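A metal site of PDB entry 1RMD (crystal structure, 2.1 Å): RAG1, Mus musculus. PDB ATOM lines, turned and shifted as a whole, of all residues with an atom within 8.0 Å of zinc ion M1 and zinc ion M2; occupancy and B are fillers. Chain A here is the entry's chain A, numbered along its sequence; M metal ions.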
ATOM      1  N   ASN A   1     -19.785  26.683   3.485  1.00  0.00           N
ATOM      2  CA  ASN A   1     -19.364  26.214   2.122  1.00  0.00           C
ATOM      3  C   ASN A   1     -19.789  27.157   0.990  1.00  0.00           C
ATOM      4  O   ASN A   1     -20.299  28.267   1.242  1.00  0.00           O
ATOM      5  CB  ASN A   1     -19.927  24.817   1.860  1.00  0.00           C
ATOM      6  CG  ASN A   1     -21.405  24.698   2.171  1.00  0.00           C
ATOM      7  OD1 ASN A   1     -22.068  25.684   2.494  1.00  0.00           O
ATOM      8  ND2 ASN A   1     -21.937  23.482   2.071  1.00  0.00           N
ATOM      9  N   CYS A   2     -19.570  26.731  -0.253  1.00  0.00           N
ATOM     10  CA  CYS A   2     -19.959  27.542  -1.415  1.00  0.00           C
ATOM     11  C   CYS A   2     -21.468  27.524  -1.632  1.00  0.00           C
ATOM     12  O   CYS A   2     -21.990  28.186  -2.524  1.00  0.00           O
ATOM     13  CB  CYS A   2     -19.246  27.057  -2.691  1.00  0.00           C
ATOM     14  SG  CYS A   2     -19.477  25.323  -3.085  1.00  0.00           S
ATOM     15  N   SER A   3     -22.160  26.737  -0.813  1.00  0.00           N
ATOM     16  CA  SER A   3     -23.615  26.603  -0.862  1.00  0.00           C
ATOM     17  C   SER A   3     -24.257  27.919  -0.407  1.00  0.00           C
ATOM     18  O   SER A   3     -25.420  28.190  -0.713  1.00  0.00           O
ATOM     19  CB  SER A   3     -24.046  25.455   0.059  1.00  0.00           C
ATOM     20  OG  SER A   3     -25.301  24.888  -0.321  1.00  0.00           O
ATOM     21  N   LYS A   4     -23.489  28.718   0.341  1.00  0.00           N
ATOM     22  CA  LYS A   4     -23.947  30.028   0.829  1.00  0.00           C
ATOM     23  C   LYS A   4     -23.927  31.043  -0.301  1.00  0.00           C
ATOM     24  O   LYS A   4     -24.586  32.075  -0.214  1.00  0.00           O
ATOM     25  CB  LYS A   4     -22.999  30.563   1.911  1.00  0.00           C
ATOM     26  CG  LYS A   4     -23.147  29.910   3.253  1.00  0.00           C
ATOM     27  CD  LYS A   4     -22.303  30.602   4.291  1.00  0.00           C
ATOM     28  CE  LYS A   4     -22.994  30.574   5.615  1.00  0.00           C
ATOM     29  NZ  LYS A   4     -22.118  31.137   6.633  1.00  0.00           N
ATOM     30  N   ILE A   5     -23.127  30.740  -1.319  1.00  0.00           N
ATOM     31  CA  ILE A   5     -22.945  31.625  -2.464  1.00  0.00           C
ATOM     32  C   ILE A   5     -23.372  31.046  -3.809  1.00  0.00           C
ATOM     33  O   ILE A   5     -23.482  31.799  -4.799  1.00  0.00           O
ATOM     34  CB  ILE A   5     -21.458  32.071  -2.569  1.00  0.00           C
ATOM     35  CG1 ILE A   5     -20.507  30.883  -2.374  1.00  0.00           C
ATOM     36  CG2 ILE A   5     -21.159  33.162  -1.550  1.00  0.00           C
ATOM     37  CD1 ILE A   5     -19.053  31.199  -2.598  1.00  0.00           C
ATOM     38  N   HIS A   6     -23.602  29.734  -3.853  1.00  0.00           N
ATOM     39  CA  HIS A   6     -23.985  29.058  -5.083  1.00  0.00           C
ATOM     40  C   HIS A   6     -25.435  28.586  -5.126  1.00  0.00           C
ATOM     41  O   HIS A   6     -26.049  28.342  -4.097  1.00  0.00           O
ATOM     42  CB  HIS A   6     -23.047  27.881  -5.318  1.00  0.00           C
ATOM     43  CG  HIS A   6     -21.638  28.294  -5.656  1.00  0.00           C
ATOM     44  ND1 HIS A   6     -20.618  27.364  -5.708  1.00  0.00           N
ATOM     45  CD2 HIS A   6     -21.149  29.531  -5.900  1.00  0.00           C
ATOM     46  CE1 HIS A   6     -19.531  28.068  -5.977  1.00  0.00           C
ATOM     47  NE2 HIS A   6     -19.797  29.381  -6.102  1.00  0.00           N
ATOM     48  N   LEU A   7     -25.998  28.475  -6.333  1.00  0.00           N
ATOM     49  CA  LEU A   7     -27.366  28.016  -6.487  1.00  0.00           C
ATOM     50  C   LEU A   7     -27.449  26.507  -6.741  1.00  0.00           C
ATOM     51  O   LEU A   7     -26.631  25.952  -7.484  1.00  0.00           O
ATOM     52  CB  LEU A   7     -28.042  28.789  -7.617  1.00  0.00           C
ATOM     53  CG  LEU A   7     -29.235  29.694  -7.255  1.00  0.00           C
ATOM     54  CD1 LEU A   7     -28.972  30.546  -5.989  1.00  0.00           C
ATOM     55  CD2 LEU A   7     -29.543  30.574  -8.462  1.00  0.00           C
ATOM     56  N   SER A   8     -28.397  25.841  -6.086  1.00  0.00           N
ATOM     57  CA  SER A   8     -28.615  24.398  -6.250  1.00  0.00           C
ATOM     58  C   SER A   8     -29.372  24.148  -7.539  1.00  0.00           C
ATOM     59  O   SER A   8     -30.294  24.908  -7.886  1.00  0.00           O
ATOM     60  CB  SER A   8     -29.449  23.840  -5.090  1.00  0.00           C
ATOM     61  OG  SER A   8     -30.007  22.576  -5.440  1.00  0.00           O
ATOM     62  N   SER A  25     -23.511  22.071 -14.443  1.00  0.00           N
ATOM     63  CA  SER A  25     -23.113  21.999 -13.030  1.00  0.00           C
ATOM     64  C   SER A  25     -21.579  21.966 -12.810  1.00  0.00           C
ATOM     65  O   SER A  25     -20.819  21.509 -13.662  1.00  0.00           O
ATOM     66  CB  SER A  25     -23.737  20.751 -12.370  1.00  0.00           C
ATOM     67  OG  SER A  25     -25.138  20.703 -12.528  1.00  0.00           O
ATOM     68  N   CYS A  26     -21.127  22.474 -11.675  1.00  0.00           N
ATOM     69  CA  CYS A  26     -19.714  22.462 -11.337  1.00  0.00           C
ATOM     70  C   CYS A  26     -19.361  21.021 -10.968  1.00  0.00           C
ATOM     71  O   CYS A  26     -19.960  20.445 -10.077  1.00  0.00           O
ATOM     72  CB  CYS A  26     -19.451  23.381 -10.134  1.00  0.00           C
ATOM     73  SG  CYS A  26     -17.866  23.096  -9.372  1.00  0.00           S
ATOM     74  N   GLN A  27     -18.372  20.456 -11.649  1.00  0.00           N
ATOM     75  CA  GLN A  27     -17.988  19.057 -11.400  1.00  0.00           C
ATOM     76  C   GLN A  27     -17.371  18.722 -10.033  1.00  0.00           C
ATOM     77  O   GLN A  27     -17.172  17.559  -9.716  1.00  0.00           O
ATOM     78  CB  GLN A  27     -17.167  18.484 -12.558  1.00  0.00           C
ATOM     79  CG  GLN A  27     -17.937  18.452 -13.884  1.00  0.00           C
ATOM     80  CD  GLN A  27     -19.316  17.822 -13.762  1.00  0.00           C
ATOM     81  OE1 GLN A  27     -19.449  16.613 -13.627  1.00  0.00           O
ATOM     82  NE2 GLN A  27     -20.346  18.645 -13.813  1.00  0.00           N
ATOM     83  N   ILE A  28     -17.105  19.768  -9.246  1.00  0.00           N
ATOM     84  CA  ILE A  28     -16.594  19.621  -7.874  1.00  0.00           C
ATOM     85  C   ILE A  28     -17.742  19.824  -6.872  1.00  0.00           C
ATOM     86  O   ILE A  28     -18.183  18.895  -6.237  1.00  0.00           O
ATOM     87  CB  ILE A  28     -15.485  20.645  -7.576  1.00  0.00           C
ATOM     88  CG1 ILE A  28     -14.192  20.214  -8.270  1.00  0.00           C
ATOM     89  CG2 ILE A  28     -15.236  20.764  -6.066  1.00  0.00           C
ATOM     90  CD1 ILE A  28     -13.103  21.279  -8.275  1.00  0.00           C
ATOM     91  N   CYS A  29     -18.276  21.035  -6.804  1.00  0.00           N
ATOM     92  CA  CYS A  29     -19.337  21.363  -5.871  1.00  0.00           C
ATOM     93  C   CYS A  29     -20.758  20.967  -6.282  1.00  0.00           C
ATOM     94  O   CYS A  29     -21.652  20.944  -5.431  1.00  0.00           O
ATOM     95  CB  CYS A  29     -19.283  22.859  -5.502  1.00  0.00           C
ATOM     96  SG  CYS A  29     -19.934  24.084  -6.676  1.00  0.00           S
ATOM     97  N   GLU A  30     -20.975  20.647  -7.556  1.00  0.00           N
ATOM     98  CA  GLU A  30     -22.300  20.248  -8.057  1.00  0.00           C
ATOM     99  C   GLU A  30     -23.395  21.324  -8.133  1.00  0.00           C
ATOM    100  O   GLU A  30     -24.543  21.044  -8.465  1.00  0.00           O
ATOM    101  CB  GLU A  30     -22.826  19.032  -7.301  1.00  0.00           C
ATOM    102  CG  GLU A  30     -22.086  17.781  -7.691  1.00  0.00           C
ATOM    103  CD  GLU A  30     -22.596  16.555  -6.970  1.00  0.00           C
ATOM    104  OE1 GLU A  30     -23.811  16.444  -6.729  1.00  0.00           O
ATOM    105  OE2 GLU A  30     -21.758  15.695  -6.662  1.00  0.00           O
ATOM    106  N   HIS A  31     -23.041  22.554  -7.816  1.00  0.00           N
ATOM    107  CA  HIS A  31     -24.033  23.625  -7.899  1.00  0.00           C
ATOM    108  C   HIS A  31     -24.103  24.091  -9.356  1.00  0.00           C
ATOM    109  O   HIS A  31     -23.340  23.584 -10.205  1.00  0.00           O
ATOM    110  CB  HIS A  31     -23.605  24.786  -7.006  1.00  0.00           C
ATOM    111  CG  HIS A  31     -23.590  24.444  -5.550  1.00  0.00           C
ATOM    112  ND1 HIS A  31     -22.462  24.630  -4.795  1.00  0.00           N
ATOM    113  CD2 HIS A  31     -24.616  24.070  -4.755  1.00  0.00           C
ATOM    114  CE1 HIS A  31     -22.830  24.369  -3.554  1.00  0.00           C
ATOM    115  NE2 HIS A  31     -24.131  24.033  -3.491  1.00  0.00           N
ATOM    116  N   ILE A  32     -25.030  24.993  -9.672  1.00  0.00           N
ATOM    117  CA  ILE A  32     -25.068  25.555 -11.023  1.00  0.00           C
ATOM    118  C   ILE A  32     -23.734  26.329 -11.146  1.00  0.00           C
ATOM    119  O   ILE A  32     -23.369  27.105 -10.233  1.00  0.00           O
ATOM    120  CB  ILE A  32     -26.226  26.553 -11.213  1.00  0.00           C
ATOM    121  CG1 ILE A  32     -27.556  25.859 -10.971  1.00  0.00           C
ATOM    122  CG2 ILE A  32     -26.194  27.121 -12.623  1.00  0.00           C
ATOM    123  CD1 ILE A  32     -28.768  26.786 -11.078  1.00  0.00           C
ATOM    124  N   LEU A  33     -22.982  26.098 -12.217  1.00  0.00           N
ATOM    125  CA  LEU A  33     -21.687  26.791 -12.384  1.00  0.00           C
ATOM    126  C   LEU A  33     -21.754  28.298 -12.064  1.00  0.00           C
ATOM    127  O   LEU A  33     -22.623  29.019 -12.569  1.00  0.00           O
ATOM    128  CB  LEU A  33     -21.169  26.641 -13.826  1.00  0.00           C
ATOM    129  CG  LEU A  33     -20.703  25.259 -14.269  1.00  0.00           C
ATOM    130  CD1 LEU A  33     -20.826  25.127 -15.784  1.00  0.00           C
ATOM    131  CD2 LEU A  33     -19.298  25.032 -13.801  1.00  0.00           C
ATOM    132  N   ALA A  34     -20.841  28.764 -11.232  1.00  0.00           N
ATOM    133  CA  ALA A  34     -20.803  30.178 -10.908  1.00  0.00           C
ATOM    134  C   ALA A  34     -19.438  30.607 -11.395  1.00  0.00           C
ATOM    135  O   ALA A  34     -18.445  30.135 -10.871  1.00  0.00           O
ATOM    136  CB  ALA A  34     -20.932  30.390  -9.386  1.00  0.00           C
ATOM    137  N   ASP A  35     -19.396  31.487 -12.402  1.00  0.00           N
ATOM    138  CA  ASP A  35     -18.135  31.962 -13.008  1.00  0.00           C
ATOM    139  C   ASP A  35     -17.361  30.757 -13.507  1.00  0.00           C
ATOM    140  O   ASP A  35     -16.271  30.450 -13.011  1.00  0.00           O
ATOM    141  CB  ASP A  35     -17.281  32.714 -11.979  1.00  0.00           C
ATOM    142  CG  ASP A  35     -16.150  33.516 -12.604  1.00  0.00           C
ATOM    143  OD1 ASP A  35     -16.177  33.716 -13.837  1.00  0.00           O
ATOM    144  OD2 ASP A  35     -15.244  33.940 -11.867  1.00  0.00           O
ATOM    145  N   LEU A  44     -15.827  21.509 -16.864  1.00  0.00           N
ATOM    146  CA  LEU A  44     -16.211  22.749 -16.186  1.00  0.00           C
ATOM    147  C   LEU A  44     -16.243  22.767 -14.649  1.00  0.00           C
ATOM    148  O   LEU A  44     -16.622  21.775 -14.015  1.00  0.00           O
ATOM    149  CB  LEU A  44     -17.567  23.213 -16.735  1.00  0.00           C
ATOM    150  CG  LEU A  44     -17.637  23.396 -18.258  1.00  0.00           C
ATOM    151  CD1 LEU A  44     -18.975  23.895 -18.659  1.00  0.00           C
ATOM    152  CD2 LEU A  44     -16.557  24.359 -18.731  1.00  0.00           C
ATOM    153  N   PHE A  45     -15.827  23.886 -14.059  1.00  0.00           N
ATOM    154  CA  PHE A  45     -15.810  24.092 -12.591  1.00  0.00           C
ATOM    155  C   PHE A  45     -15.914  25.591 -12.310  1.00  0.00           C
ATOM    156  O   PHE A  45     -15.444  26.408 -13.107  1.00  0.00           O
ATOM    157  CB  PHE A  45     -14.497  23.621 -11.947  1.00  0.00           C
ATOM    158  CG  PHE A  45     -14.065  22.276 -12.371  1.00  0.00           C
ATOM    159  CD1 PHE A  45     -13.285  22.109 -13.513  1.00  0.00           C
ATOM    160  CD2 PHE A  45     -14.473  21.146 -11.671  1.00  0.00           C
ATOM    161  CE1 PHE A  45     -12.924  20.841 -13.967  1.00  0.00           C
ATOM    162  CE2 PHE A  45     -14.116  19.861 -12.111  1.00  0.00           C
ATOM    163  CZ  PHE A  45     -13.328  19.719 -13.278  1.00  0.00           C
ATOM    164  N   CYS A  46     -16.513  25.960 -11.166  1.00  0.00           N
ATOM    165  CA  CYS A  46     -16.608  27.373 -10.768  1.00  0.00           C
ATOM    166  C   CYS A  46     -15.151  27.786 -10.583  1.00  0.00           C
ATOM    167  O   CYS A  46     -14.381  27.009 -10.021  1.00  0.00           O
ATOM    168  CB  CYS A  46     -17.301  27.540  -9.403  1.00  0.00           C
ATOM    169  SG  CYS A  46     -18.832  26.606  -9.062  1.00  0.00           S
ATOM    170  N   ARG A  47     -14.771  28.985 -11.041  1.00  0.00           N
ATOM    171  CA  ARG A  47     -13.389  29.477 -10.877  1.00  0.00           C
ATOM    172  C   ARG A  47     -12.795  29.223  -9.473  1.00  0.00           C
ATOM    173  O   ARG A  47     -11.645  28.829  -9.381  1.00  0.00           O
ATOM    174  CB  ARG A  47     -13.318  30.988 -11.175  1.00  0.00           C
ATOM    175  CG  ARG A  47     -12.014  31.705 -10.764  1.00  0.00           C
ATOM    176  CD  ARG A  47     -10.942  31.719 -11.856  1.00  0.00           C
ATOM    177  NE  ARG A  47     -11.406  32.211 -13.156  1.00  0.00           N
ATOM    178  CZ  ARG A  47     -12.168  33.275 -13.331  1.00  0.00           C
ATOM    179  NH1 ARG A  47     -12.554  33.996 -12.287  1.00  0.00           N
ATOM    180  NH2 ARG A  47     -12.613  33.592 -14.544  1.00  0.00           N
ATOM    181  N   ILE A  48     -13.562  29.412  -8.410  1.00  0.00           N
ATOM    182  CA  ILE A  48     -13.001  29.181  -7.084  1.00  0.00           C
ATOM    183  C   ILE A  48     -12.889  27.715  -6.710  1.00  0.00           C
ATOM    184  O   ILE A  48     -11.961  27.333  -5.989  1.00  0.00           O
ATOM    185  CB  ILE A  48     -13.778  29.896  -5.930  1.00  0.00           C
ATOM    186  CG1 ILE A  48     -15.173  29.300  -5.756  1.00  0.00           C
ATOM    187  CG2 ILE A  48     -13.822  31.403  -6.168  1.00  0.00           C
ATOM    188  CD1 ILE A  48     -15.958  29.851  -4.553  1.00  0.00           C
ATOM    189  N   CYS A  49     -13.800  26.891  -7.191  1.00  0.00           N
ATOM    190  CA  CYS A  49     -13.745  25.481  -6.801  1.00  0.00           C
ATOM    191  C   CYS A  49     -12.520  24.783  -7.370  1.00  0.00           C
ATOM    192  O   CYS A  49     -11.816  24.046  -6.645  1.00  0.00           O
ATOM    193  CB  CYS A  49     -15.023  24.756  -7.198  1.00  0.00           C
ATOM    194  SG  CYS A  49     -16.498  25.420  -6.365  1.00  0.00           S
ATOM    195  N   ILE A  50     -12.219  25.060  -8.637  1.00  0.00           N
ATOM    196  CA  ILE A  50     -11.093  24.427  -9.292  1.00  0.00           C
ATOM    197  C   ILE A  50      -9.725  24.895  -8.754  1.00  0.00           C
ATOM    198  O   ILE A  50      -8.877  24.061  -8.424  1.00  0.00           O
ATOM    199  CB  ILE A  50     -11.210  24.552 -10.845  1.00  0.00           C
ATOM    200  CG1 ILE A  50     -10.107  23.731 -11.510  1.00  0.00           C
ATOM    201  CG2 ILE A  50     -11.229  26.013 -11.275  1.00  0.00           C
ATOM    202  CD1 ILE A  50     -10.112  22.261 -11.123  1.00  0.00           C
ATOM    203  N   ARG A  52      -8.964  25.890  -5.854  1.00  0.00           N
ATOM    204  CA  ARG A  52      -8.667  25.343  -4.541  1.00  0.00           C
ATOM    205  C   ARG A  52      -8.231  23.895  -4.664  1.00  0.00           C
ATOM    206  O   ARG A  52      -7.305  23.463  -3.977  1.00  0.00           O
ATOM    207  CB  ARG A  52      -9.872  25.492  -3.598  1.00  0.00           C
ATOM    208  CG  ARG A  52      -9.681  24.899  -2.188  1.00  0.00           C
ATOM    209  CD  ARG A  52     -10.104  23.420  -2.090  1.00  0.00           C
ATOM    210  NE  ARG A  52     -11.380  23.181  -2.778  1.00  0.00           N
ATOM    211  CZ  ARG A  52     -11.945  21.994  -2.979  1.00  0.00           C
ATOM    212  NH1 ARG A  52     -11.362  20.871  -2.545  1.00  0.00           N
ATOM    213  NH2 ARG A  52     -13.052  21.897  -3.701  1.00  0.00           N
HETATM  214 ZN    ZN M   1     -18.101  24.860  -7.867  1.00  0.00          ZN
HETATM  215 ZN    ZN M   2     -20.655  25.619  -5.052  1.00  0.00          ZN
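The side-chain sulfur (SG) of Cys 26 lies close to the backbone NH (N) of Ile 28. N of Cys 26 sits at hydrogen-bond distance from O of His 31, at 2.9 Å. The backbone NH of Ala 34 lies close to the side-chain sulfur of Cys 46 (3.7 Å). The side-chain hydroxyl (OG) of Ser 3 lies within hydrogen-bond range of a ring nitrogen (NE2) of His 31, at 3.5 Å.
Five residues have an atom within 4 Å of zinc ion M1: His 6, Cys 26, Cys 29, Cys 46 and Cys 49.
Four residues have an atom within 4 Å of zinc ion M2: Cys 2, His 6, Cys 29 and His 31.
Zinc ion M1 is bound by SG of Cys 46 (2.2 Å), SG of Cys 49 (2.3 Å), SG of Cys 29 (2.3 Å) and SG of Cys 26 (2.3 Å). Zinc ion M1 has four donor atoms within binding distance.
Zinc ion M2 is bound by ND1 of His 6 (1.9 Å). Zinc ion M2 is bound by ND1 of His 31 (2.1 Å). Zinc ion M2 is bound by SG of Cys 2, at 2.3 Å. SG of Cys 29 is bound to zinc ion M2 (2.3 Å). Zinc ion M2 has four donor atoms within binding distance.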
